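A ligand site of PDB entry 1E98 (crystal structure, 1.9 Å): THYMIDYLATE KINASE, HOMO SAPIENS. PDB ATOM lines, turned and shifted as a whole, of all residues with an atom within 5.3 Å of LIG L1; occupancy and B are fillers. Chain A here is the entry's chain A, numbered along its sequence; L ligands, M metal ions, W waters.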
ATOM      1  N   ASP A  18     -12.160  31.848   5.513  1.00  0.00           N
ATOM      2  CA  ASP A  18     -13.515  32.211   5.088  1.00  0.00           C
ATOM      3  C   ASP A  18     -13.544  33.636   4.584  1.00  0.00           C
ATOM      4  O   ASP A  18     -13.007  34.527   5.242  1.00  0.00           O
ATOM      5  CB  ASP A  18     -14.455  31.956   6.285  1.00  0.00           C
ATOM      6  CG  ASP A  18     -15.908  32.204   5.935  1.00  0.00           C
ATOM      7  OD1 ASP A  18     -16.407  31.661   4.927  1.00  0.00           O
ATOM      8  OD2 ASP A  18     -16.558  32.981   6.653  1.00  0.00           O
ATOM      9  N   LYS A  22     -11.253  32.921  -2.342  1.00  0.00           N
ATOM     10  CA  LYS A  22     -10.914  31.770  -3.190  1.00  0.00           C
ATOM     11  C   LYS A  22     -11.644  31.804  -4.517  1.00  0.00           C
ATOM     12  O   LYS A  22     -11.090  31.570  -5.583  1.00  0.00           O
ATOM     13  CB  LYS A  22     -11.224  30.471  -2.413  1.00  0.00           C
ATOM     14  CG  LYS A  22     -10.409  30.366  -1.093  1.00  0.00           C
ATOM     15  CD  LYS A  22     -10.773  29.129  -0.276  1.00  0.00           C
ATOM     16  CE  LYS A  22     -12.187  29.116   0.277  1.00  0.00           C
ATOM     17  NZ  LYS A  22     -12.498  30.235   1.220  1.00  0.00           N
ATOM     18  N   SER A  23     -12.961  31.982  -4.492  1.00  0.00           N
ATOM     19  CA  SER A  23     -13.794  31.983  -5.685  1.00  0.00           C
ATOM     20  C   SER A  23     -13.530  33.203  -6.551  1.00  0.00           C
ATOM     21  O   SER A  23     -13.318  33.036  -7.739  1.00  0.00           O
ATOM     22  CB  SER A  23     -15.286  31.985  -5.297  1.00  0.00           C
ATOM     23  OG  SER A  23     -15.397  30.788  -4.542  1.00  0.00           O
ATOM     24  N   PHE A  45     -14.528  22.455  -5.626  1.00  0.00           N
ATOM     25  CA  PHE A  45     -15.049  21.366  -4.832  1.00  0.00           C
ATOM     26  C   PHE A  45     -15.708  21.974  -3.593  1.00  0.00           C
ATOM     27  O   PHE A  45     -15.144  22.912  -3.055  1.00  0.00           O
ATOM     28  CB  PHE A  45     -13.969  20.342  -4.473  1.00  0.00           C
ATOM     29  CG  PHE A  45     -13.471  19.585  -5.687  1.00  0.00           C
ATOM     30  CD1 PHE A  45     -14.222  18.533  -6.218  1.00  0.00           C
ATOM     31  CD2 PHE A  45     -12.266  19.975  -6.270  1.00  0.00           C
ATOM     32  CE1 PHE A  45     -13.725  17.868  -7.338  1.00  0.00           C
ATOM     33  CE2 PHE A  45     -11.793  19.288  -7.383  1.00  0.00           C
ATOM     34  CZ  PHE A  45     -12.532  18.231  -7.922  1.00  0.00           C
ATOM     35  N   PRO A  46     -16.822  21.422  -3.192  1.00  0.00           N
ATOM     36  CA  PRO A  46     -17.483  20.339  -3.861  1.00  0.00           C
ATOM     37  C   PRO A  46     -18.041  20.719  -5.231  1.00  0.00           C
ATOM     38  O   PRO A  46     -18.352  21.881  -5.574  1.00  0.00           O
ATOM     39  CB  PRO A  46     -18.674  19.969  -2.943  1.00  0.00           C
ATOM     40  CG  PRO A  46     -18.980  21.305  -2.353  1.00  0.00           C
ATOM     41  CD  PRO A  46     -17.642  21.944  -2.041  1.00  0.00           C
ATOM     42  N   ARG A  48     -21.034  20.332  -7.123  1.00  0.00           N
ATOM     43  CA  ARG A  48     -22.401  19.974  -6.775  1.00  0.00           C
ATOM     44  C   ARG A  48     -23.294  19.448  -7.869  1.00  0.00           C
ATOM     45  O   ARG A  48     -24.436  19.102  -7.554  1.00  0.00           O
ATOM     46  CB  ARG A  48     -23.080  21.226  -6.157  1.00  0.00           C
ATOM     47  CG  ARG A  48     -22.219  21.784  -5.013  1.00  0.00           C
ATOM     48  CD  ARG A  48     -22.891  23.019  -4.436  1.00  0.00           C
ATOM     49  NE  ARG A  48     -22.096  23.665  -3.385  1.00  0.00           N
ATOM     50  CZ  ARG A  48     -22.632  24.015  -2.202  1.00  0.00           C
ATOM     51  NH1 ARG A  48     -23.912  23.775  -1.936  1.00  0.00           N
ATOM     52  NH2 ARG A  48     -21.895  24.606  -1.271  1.00  0.00           N
ATOM     53  N   LEU A  60     -24.697  20.824   3.172  1.00  0.00           N
ATOM     54  CA  LEU A  60     -24.151  22.129   3.489  1.00  0.00           C
ATOM     55  C   LEU A  60     -25.241  23.182   3.691  1.00  0.00           C
ATOM     56  O   LEU A  60     -24.986  24.156   4.397  1.00  0.00           O
ATOM     57  CB  LEU A  60     -23.190  22.621   2.403  1.00  0.00           C
ATOM     58  CG  LEU A  60     -21.911  21.739   2.300  1.00  0.00           C
ATOM     59  CD1 LEU A  60     -21.247  21.967   0.950  1.00  0.00           C
ATOM     60  CD2 LEU A  60     -21.006  22.018   3.496  1.00  0.00           C
ATOM     61  N   PHE A  75     -17.361  13.698   0.275  1.00  0.00           N
ATOM     62  CA  PHE A  75     -16.593  14.840  -0.193  1.00  0.00           C
ATOM     63  C   PHE A  75     -15.352  14.349  -0.975  1.00  0.00           C
ATOM     64  O   PHE A  75     -14.971  14.894  -2.003  1.00  0.00           O
ATOM     65  CB  PHE A  75     -16.082  15.699   1.002  1.00  0.00           C
ATOM     66  CG  PHE A  75     -17.006  16.834   1.376  1.00  0.00           C
ATOM     67  CD1 PHE A  75     -17.206  17.898   0.499  1.00  0.00           C
ATOM     68  CD2 PHE A  75     -17.691  16.840   2.605  1.00  0.00           C
ATOM     69  CE1 PHE A  75     -18.065  18.938   0.829  1.00  0.00           C
ATOM     70  CE2 PHE A  75     -18.511  17.894   2.943  1.00  0.00           C
ATOM     71  CZ  PHE A  75     -18.713  18.956   2.051  1.00  0.00           C
ATOM     72  N   SER A  76     -14.666  13.325  -0.452  1.00  0.00           N
ATOM     73  CA  SER A  76     -13.489  12.777  -1.158  1.00  0.00           C
ATOM     74  C   SER A  76     -13.940  12.085  -2.438  1.00  0.00           C
ATOM     75  O   SER A  76     -13.327  12.238  -3.509  1.00  0.00           O
ATOM     76  CB  SER A  76     -12.743  11.803  -0.233  1.00  0.00           C
ATOM     77  OG  SER A  76     -11.716  11.133  -0.978  1.00  0.00           O
ATOM     78  N   ARG A  79     -14.221  14.240  -5.320  1.00  0.00           N
ATOM     79  CA  ARG A  79     -12.951  14.536  -5.999  1.00  0.00           C
ATOM     80  C   ARG A  79     -12.549  13.395  -6.944  1.00  0.00           C
ATOM     81  O   ARG A  79     -12.214  13.640  -8.092  1.00  0.00           O
ATOM     82  CB  ARG A  79     -11.780  14.849  -5.085  1.00  0.00           C
ATOM     83  CG  ARG A  79     -11.962  16.224  -4.388  1.00  0.00           C
ATOM     84  CD  ARG A  79     -10.871  16.360  -3.347  1.00  0.00           C
ATOM     85  NE  ARG A  79     -11.035  15.769  -2.039  1.00  0.00           N
ATOM     86  CZ  ARG A  79     -11.884  16.259  -1.095  1.00  0.00           C
ATOM     87  NH1 ARG A  79     -12.730  17.255  -1.388  1.00  0.00           N
ATOM     88  NH2 ARG A  79     -11.951  15.704   0.108  1.00  0.00           N
ATOM     89  N   ASP A  99     -10.880  25.684  -6.949  1.00  0.00           N
ATOM     90  CA  ASP A  99     -11.400  26.404  -5.805  1.00  0.00           C
ATOM     91  C   ASP A  99     -11.703  25.384  -4.698  1.00  0.00           C
ATOM     92  O   ASP A  99     -12.790  24.842  -4.757  1.00  0.00           O
ATOM     93  CB  ASP A  99     -12.694  27.097  -6.263  1.00  0.00           C
ATOM     94  CG  ASP A  99     -13.346  28.019  -5.256  1.00  0.00           C
ATOM     95  OD1 ASP A  99     -12.946  27.972  -4.061  1.00  0.00           O
ATOM     96  OD2 ASP A  99     -14.281  28.758  -5.713  1.00  0.00           O
ATOM     97  N   ARG A 100     -10.765  25.167  -3.811  1.00  0.00           N
ATOM     98  CA  ARG A 100     -10.821  24.179  -2.758  1.00  0.00           C
ATOM     99  C   ARG A 100     -10.472  22.765  -3.305  1.00  0.00           C
ATOM    100  O   ARG A 100     -10.901  22.366  -4.382  1.00  0.00           O
ATOM    101  CB  ARG A 100     -12.123  24.070  -1.996  1.00  0.00           C
ATOM    102  CG  ARG A 100     -12.485  25.306  -1.130  1.00  0.00           C
ATOM    103  CD  ARG A 100     -13.708  24.818  -0.297  1.00  0.00           C
ATOM    104  NE  ARG A 100     -14.323  25.932   0.378  1.00  0.00           N
ATOM    105  CZ  ARG A 100     -13.972  26.466   1.545  1.00  0.00           C
ATOM    106  NH1 ARG A 100     -12.959  25.998   2.245  1.00  0.00           N
ATOM    107  NH2 ARG A 100     -14.651  27.520   2.007  1.00  0.00           N
ATOM    108  N   TYR A 101      -9.758  22.010  -2.468  1.00  0.00           N
ATOM    109  CA  TYR A 101      -9.431  20.618  -2.821  1.00  0.00           C
ATOM    110  C   TYR A 101      -9.400  19.732  -1.586  1.00  0.00           C
ATOM    111  O   TYR A 101     -10.191  19.875  -0.632  1.00  0.00           O
ATOM    112  CB  TYR A 101      -8.081  20.628  -3.545  1.00  0.00           C
ATOM    113  CG  TYR A 101      -7.628  19.455  -4.390  1.00  0.00           C
ATOM    114  CD1 TYR A 101      -8.463  18.947  -5.364  1.00  0.00           C
ATOM    115  CD2 TYR A 101      -6.388  18.832  -4.211  1.00  0.00           C
ATOM    116  CE1 TYR A 101      -8.090  17.908  -6.184  1.00  0.00           C
ATOM    117  CE2 TYR A 101      -5.977  17.767  -5.039  1.00  0.00           C
ATOM    118  CZ  TYR A 101      -6.810  17.349  -6.027  1.00  0.00           C
ATOM    119  OH  TYR A 101      -6.544  16.292  -6.880  1.00  0.00           O
ATOM    120  N   SER A 104      -9.249  21.410   2.167  1.00  0.00           N
ATOM    121  CA  SER A 104     -10.513  21.730   2.769  1.00  0.00           C
ATOM    122  C   SER A 104     -11.205  20.449   3.299  1.00  0.00           C
ATOM    123  O   SER A 104     -11.772  20.444   4.405  1.00  0.00           O
ATOM    124  CB  SER A 104     -11.472  22.460   1.832  1.00  0.00           C
ATOM    125  OG  SER A 104     -11.097  23.827   1.744  1.00  0.00           O
ATOM    126  N   GLY A 105     -11.146  19.405   2.502  1.00  0.00           N
ATOM    127  CA  GLY A 105     -11.753  18.142   2.946  1.00  0.00           C
ATOM    128  C   GLY A 105     -11.242  17.748   4.325  1.00  0.00           C
ATOM    129  O   GLY A 105     -12.021  17.275   5.166  1.00  0.00           O
ATOM    130  N   PHE A 108     -11.948  20.649   7.367  1.00  0.00           N
ATOM    131  CA  PHE A 108     -13.334  20.803   7.781  1.00  0.00           C
ATOM    132  C   PHE A 108     -13.826  19.588   8.577  1.00  0.00           C
ATOM    133  O   PHE A 108     -14.441  19.808   9.632  1.00  0.00           O
ATOM    134  CB  PHE A 108     -14.236  21.123   6.577  1.00  0.00           C
ATOM    135  CG  PHE A 108     -14.125  22.651   6.428  1.00  0.00           C
ATOM    136  CD1 PHE A 108     -13.086  23.226   5.722  1.00  0.00           C
ATOM    137  CD2 PHE A 108     -15.065  23.460   7.016  1.00  0.00           C
ATOM    138  CE1 PHE A 108     -12.966  24.601   5.589  1.00  0.00           C
ATOM    139  CE2 PHE A 108     -14.950  24.847   6.881  1.00  0.00           C
ATOM    140  CZ  PHE A 108     -13.916  25.436   6.174  1.00  0.00           C
ATOM    141  N   THR A 109     -13.538  18.367   8.131  1.00  0.00           N
ATOM    142  CA  THR A 109     -13.905  17.193   8.982  1.00  0.00           C
ATOM    143  C   THR A 109     -12.970  17.145  10.189  1.00  0.00           C
ATOM    144  O   THR A 109     -13.351  16.915  11.341  1.00  0.00           O
ATOM    145  CB  THR A 109     -13.831  15.890   8.174  1.00  0.00           C
ATOM    146  OG1 THR A 109     -14.877  16.005   7.166  1.00  0.00           O
ATOM    147  CG2 THR A 109     -14.096  14.639   8.980  1.00  0.00           C
ATOM    148  N   GLU A 152     -24.901  28.546   5.583  1.00  0.00           N
ATOM    149  CA  GLU A 152     -24.535  27.154   5.384  1.00  0.00           C
ATOM    150  C   GLU A 152     -23.797  26.575   6.587  1.00  0.00           C
ATOM    151  O   GLU A 152     -23.265  27.241   7.463  1.00  0.00           O
ATOM    152  CB  GLU A 152     -23.700  26.944   4.102  1.00  0.00           C
ATOM    153  CG  GLU A 152     -24.483  26.889   2.796  1.00  0.00           C
ATOM    154  CD  GLU A 152     -23.730  26.239   1.645  1.00  0.00           C
ATOM    155  OE1 GLU A 152     -22.481  26.251   1.513  1.00  0.00           O
ATOM    156  OE2 GLU A 152     -24.397  25.624   0.758  1.00  0.00           O
ATOM    157  N   ARG A 153     -23.741  25.246   6.602  1.00  0.00           N
ATOM    158  CA  ARG A 153     -23.067  24.509   7.651  1.00  0.00           C
ATOM    159  C   ARG A 153     -21.586  24.905   7.636  1.00  0.00           C
ATOM    160  O   ARG A 153     -20.999  25.157   6.596  1.00  0.00           O
ATOM    161  CB  ARG A 153     -23.241  23.026   7.376  1.00  0.00           C
ATOM    162  CG  ARG A 153     -23.324  22.122   8.593  1.00  0.00           C
ATOM    163  CD  ARG A 153     -23.265  20.677   8.091  1.00  0.00           C
ATOM    164  NE  ARG A 153     -24.570  20.202   7.611  1.00  0.00           N
ATOM    165  CZ  ARG A 153     -25.561  19.927   8.450  1.00  0.00           C
ATOM    166  NH1 ARG A 153     -25.346  20.092   9.745  1.00  0.00           N
ATOM    167  NH2 ARG A 153     -26.716  19.466   8.048  1.00  0.00           N
ATOM    168  N   TYR A 154     -21.017  24.987   8.815  1.00  0.00           N
ATOM    169  CA  TYR A 154     -19.627  25.263   9.077  1.00  0.00           C
ATOM    170  C   TYR A 154     -19.325  26.761   9.101  1.00  0.00           C
ATOM    171  O   TYR A 154     -18.174  27.115   9.297  1.00  0.00           O
ATOM    172  CB  TYR A 154     -18.697  24.577   8.074  1.00  0.00           C
ATOM    173  CG  TYR A 154     -18.802  23.065   7.945  1.00  0.00           C
ATOM    174  CD1 TYR A 154     -19.247  22.252   8.974  1.00  0.00           C
ATOM    175  CD2 TYR A 154     -18.385  22.450   6.763  1.00  0.00           C
ATOM    176  CE1 TYR A 154     -19.329  20.877   8.856  1.00  0.00           C
ATOM    177  CE2 TYR A 154     -18.431  21.085   6.624  1.00  0.00           C
ATOM    178  CZ  TYR A 154     -18.901  20.296   7.682  1.00  0.00           C
ATOM    179  OH  TYR A 154     -18.951  18.917   7.496  1.00  0.00           O
ATOM    180  N   GLU A 155     -20.311  27.599   8.816  1.00  0.00           N
ATOM    181  CA  GLU A 155     -20.025  29.048   8.785  1.00  0.00           C
ATOM    182  C   GLU A 155     -20.229  29.702  10.141  1.00  0.00           C
ATOM    183  O   GLU A 155     -21.205  30.406  10.367  1.00  0.00           O
ATOM    184  CB  GLU A 155     -20.948  29.665   7.739  1.00  0.00           C
ATOM    185  CG  GLU A 155     -20.503  29.238   6.343  1.00  0.00           C
ATOM    186  CD  GLU A 155     -21.473  29.780   5.315  1.00  0.00           C
ATOM    187  OE1 GLU A 155     -22.643  29.328   5.304  1.00  0.00           O
ATOM    188  OE2 GLU A 155     -21.063  30.655   4.541  1.00  0.00           O
ATOM    189  N   GLN A 160     -14.670  27.699  12.359  1.00  0.00           N
ATOM    190  CA  GLN A 160     -13.685  28.124  11.345  1.00  0.00           C
ATOM    191  C   GLN A 160     -12.288  28.114  11.904  1.00  0.00           C
ATOM    192  O   GLN A 160     -11.260  27.750  11.277  1.00  0.00           O
ATOM    193  CB  GLN A 160     -14.104  29.458  10.715  1.00  0.00           C
ATOM    194  CG  GLN A 160     -15.367  29.375   9.863  1.00  0.00           C
ATOM    195  CD  GLN A 160     -15.063  28.943   8.444  1.00  0.00           C
ATOM    196  OE1 GLN A 160     -14.061  29.341   7.873  1.00  0.00           O
ATOM    197  NE2 GLN A 160     -15.920  28.126   7.855  1.00  0.00           N
HETATM  198  P1  LIG L   1     -17.525  27.000  -0.488  1.00  0.00           P
HETATM  199  O1  LIG L   1     -17.182  27.937   0.624  1.00  0.00           O
HETATM  200  O2  LIG L   1     -16.321  26.802  -1.433  1.00  0.00           O
HETATM  201  O3  LIG L   1     -18.798  27.422  -1.230  1.00  0.00           O
HETATM  202  O4  LIG L   1     -17.626  25.496   0.039  1.00  0.00           O
HETATM  203  C1  LIG L   1     -18.582  25.007   0.929  1.00  0.00           C
HETATM  204  C2  LIG L   1     -18.162  24.149   2.127  1.00  0.00           C
HETATM  205  O5  LIG L   1     -17.711  22.809   2.074  1.00  0.00           O
HETATM  206  C3  LIG L   1     -17.204  24.892   3.025  1.00  0.00           C
HETATM  207  N1  LIG L   1     -17.977  24.953   4.329  1.00  0.00           N
HETATM  208  N2  LIG L   1     -17.675  25.992   4.946  1.00  0.00           N
HETATM  209  N3  LIG L   1     -17.184  26.986   5.190  1.00  0.00           N
HETATM  210  C4  LIG L   1     -15.967  23.979   3.099  1.00  0.00           C
HETATM  211  C5  LIG L   1     -16.567  22.590   2.860  1.00  0.00           C
HETATM  212  N4  LIG L   1     -15.840  21.438   2.320  1.00  0.00           N
HETATM  213  C6  LIG L   1     -15.758  20.284   3.156  1.00  0.00           C
HETATM  214  O6  LIG L   1     -16.253  20.269   4.290  1.00  0.00           O
HETATM  215  N5  LIG L   1     -15.070  19.205   2.646  1.00  0.00           N
HETATM  216  C7  LIG L   1     -14.526  19.261   1.391  1.00  0.00           C
HETATM  217  O7  LIG L   1     -13.881  18.132   0.902  1.00  0.00           O
HETATM  218  C8  LIG L   1     -14.652  20.481   0.543  1.00  0.00           C
HETATM  219  C9  LIG L   1     -14.050  20.521  -0.826  1.00  0.00           C
HETATM  220  C10 LIG L   1     -15.342  21.568   1.060  1.00  0.00           C
HETATM  221  P1  LG2 L   2     -14.424  32.730  -0.678  1.00  0.00           P
HETATM  222  O1  LG2 L   2     -13.030  32.631  -0.170  1.00  0.00           O
HETATM  223  O2  LG2 L   2     -14.740  31.919  -1.893  1.00  0.00           O
HETATM  224  O3  LG2 L   2     -15.487  32.498   0.417  1.00  0.00           O
HETATM  225  P2  LG2 L   2     -15.323  35.093  -2.200  1.00  0.00           P
HETATM  226  O4  LG2 L   2     -16.658  34.553  -2.442  1.00  0.00           O
HETATM  227  O5  LG2 L   2     -14.329  35.216  -3.333  1.00  0.00           O
HETATM  228  O6  LG2 L   2     -14.530  34.330  -1.011  1.00  0.00           O
HETATM  229  O7  LG2 L   2     -15.369  36.555  -1.601  1.00  0.00           O
HETATM  230  C1  LG2 L   2     -16.084  36.887  -0.384  1.00  0.00           C
HETATM  231  C2  LG2 L   2     -16.675  38.285  -0.465  1.00  0.00           C
HETATM  232  O8  LG2 L   2     -15.545  39.141  -0.274  1.00  0.00           O
HETATM  233  C3  LG2 L   2     -17.328  38.682  -1.796  1.00  0.00           C
HETATM  234  O9  LG2 L   2     -18.208  39.773  -1.550  1.00  0.00           O
HETATM  235  C4  LG2 L   2     -16.112  39.244  -2.546  1.00  0.00           C
HETATM  236  O10 LG2 L   2     -16.429  40.241  -3.476  1.00  0.00           O
HETATM  237  C5  LG2 L   2     -15.341  39.923  -1.395  1.00  0.00           C
HETATM  238  N1  LG2 L   2     -13.884  39.985  -1.643  1.00  0.00           N
HETATM  239  C6  LG2 L   2     -13.111  38.981  -2.199  1.00  0.00           C
HETATM  240  N2  LG2 L   2     -11.819  39.278  -2.194  1.00  0.00           N
HETATM  241  C7  LG2 L   2     -11.745  40.564  -1.642  1.00  0.00           C
HETATM  242  C8  LG2 L   2     -10.652  41.397  -1.413  1.00  0.00           C
HETATM  243  N3  LG2 L   2      -9.407  41.139  -1.676  1.00  0.00           N
HETATM  244  N4  LG2 L   2     -11.025  42.558  -0.844  1.00  0.00           N
HETATM  245  C9  LG2 L   2     -12.266  42.928  -0.543  1.00  0.00           C
HETATM  246  N5  LG2 L   2     -13.348  42.175  -0.757  1.00  0.00           N
HETATM  247  C10 LG2 L   2     -12.993  41.028  -1.282  1.00  0.00           C
HETATM  248 MG    MG M   1     -16.149  30.548  -2.434  1.00  0.00          MG
HETATM  249  O   HOH W   1     -15.664  29.329   4.774  1.00  0.00           O
HETATM  250  O   HOH W   2     -14.561  16.902   4.061  1.00  0.00           O
HETATM  251  O   HOH W   3     -17.617  29.159  -3.094  1.00  0.00           O
HETATM  252  O   HOH W   4     -16.574  18.253   6.128  1.00  0.00           O
HETATM  253  O   HOH W   5     -16.769  30.272  -0.367  1.00  0.00           O
HETATM  254  O   HOH W   6     -16.242  25.481  -3.822  1.00  0.00           O
HETATM  255  O   HOH W   7     -18.398  28.355   2.830  1.00  0.00           O
HETATM  256  O   HOH W   8     -20.480  26.400   3.566  1.00  0.00           O
HETATM  257  O   HOH W   9     -14.740  28.843  -2.251  1.00  0.00           O
HETATM  258  O   HOH W  10     -19.820  25.648  -2.708  1.00  0.00           O
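The guanidinium group (NH1) of Arg 79 lies within hydrogen-bond range of an oxygen (O7) of LIG L1, 2.7 Å away.
NE of Arg 100 lies within salt-bridge range of O2 of LIG L1 (2.8 Å).
O7 of LIG L1 lies close to N of Gly 105, at 3.4 Å.
NE2 of Gln 160 is in hydrogen-bond range of N3 of LIG L1, at 3.2 Å.
The backbone NH (N) of Lys 22 lies within hydrogen-bond range of an oxygen (O1) of LG2 L2 (2.8 Å).
The side-chain amino group of Lys 22 lies within salt-bridge range of an oxygen (O1) of LG2 L2.
N of Ser 23 lies close to O2 of LG2 L2 (3.2 Å).
The guanidinium group (NH1) of Arg 79 is in hydrogen-bond range of the backbone carbonyl oxygen (O) of Phe 75 (3.3 Å).
NH1 of Arg 100 lies within hydrogen-bond range of OG of Ser 104 (2.9 Å).
O of Tyr 154 sits at hydrogen-bond distance from NE2 of Gln 160 (2.9 Å).
N of Phe 45 is in hydrogen-bond range of O of Asp 99 (3.1 Å).
The backbone carbonyl oxygen (O) of Leu 60 is in hydrogen-bond range of the backbone NH (N) of Arg 153 (2.8 Å).
The side-chain carboxylate (OE1) of Glu 152 lies within salt-bridge range of the guanidinium group (NH2) of Arg 48 (3.3 Å).
Merely in contact with LIG L1: Phe 45 (3.4 Å), Pro 46 (3.8 Å), Arg 48 (3.997 Å), Leu 60 (3.7 Å), Phe 75 (3.1 Å), Tyr 101 (3.9 Å), Ser 104 (3.9 Å), Phe 108 (3.2 Å), Arg 153 (3.8 Å) and Tyr 154 (3.3 Å).
Of the 22 residues printed, 14 come within 4 Å of LIG L1.
Along chain A the residues within 4 Å of LIG L1 span positions 45 to 160.
Water W10 bridges O3 of LIG L1 (2.5 Å) and NH2 of Arg 48 (2.7 Å).
Water W5 bridges O1 of LIG L1 (2.6 Å) and O3 of LG2 L2 (2.7 Å).
Water W9 lies within hydrogen-bond range of the side-chain carboxylate of Asp 99 (2.7 Å) and an oxygen (O2) of LIG L1 (2.7 Å).
Water W6 bridges an oxygen (O2) of LIG L1 (2.7 Å) and the backbone carbonyl oxygen (O) of Phe 45 (2.9 Å).
Water W2 lies within hydrogen-bond range of a nitrogen (N5) of LIG L1 (2.8 Å), the backbone carbonyl oxygen of Gly 105 (2.8 Å) and the side-chain hydroxyl of Thr 109 (3.2 Å).
Water W1 lies within hydrogen-bond range of the side-chain carboxylate (OD1) of Asp 18 (2.5 Å), a nitrogen (N3) of LIG L1 (2.8 Å), the side-chain amide nitrogen (NE2) of Gln 160 (3.3 Å) and the guanidinium group (NH2) of Arg 100 (3.5 Å).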
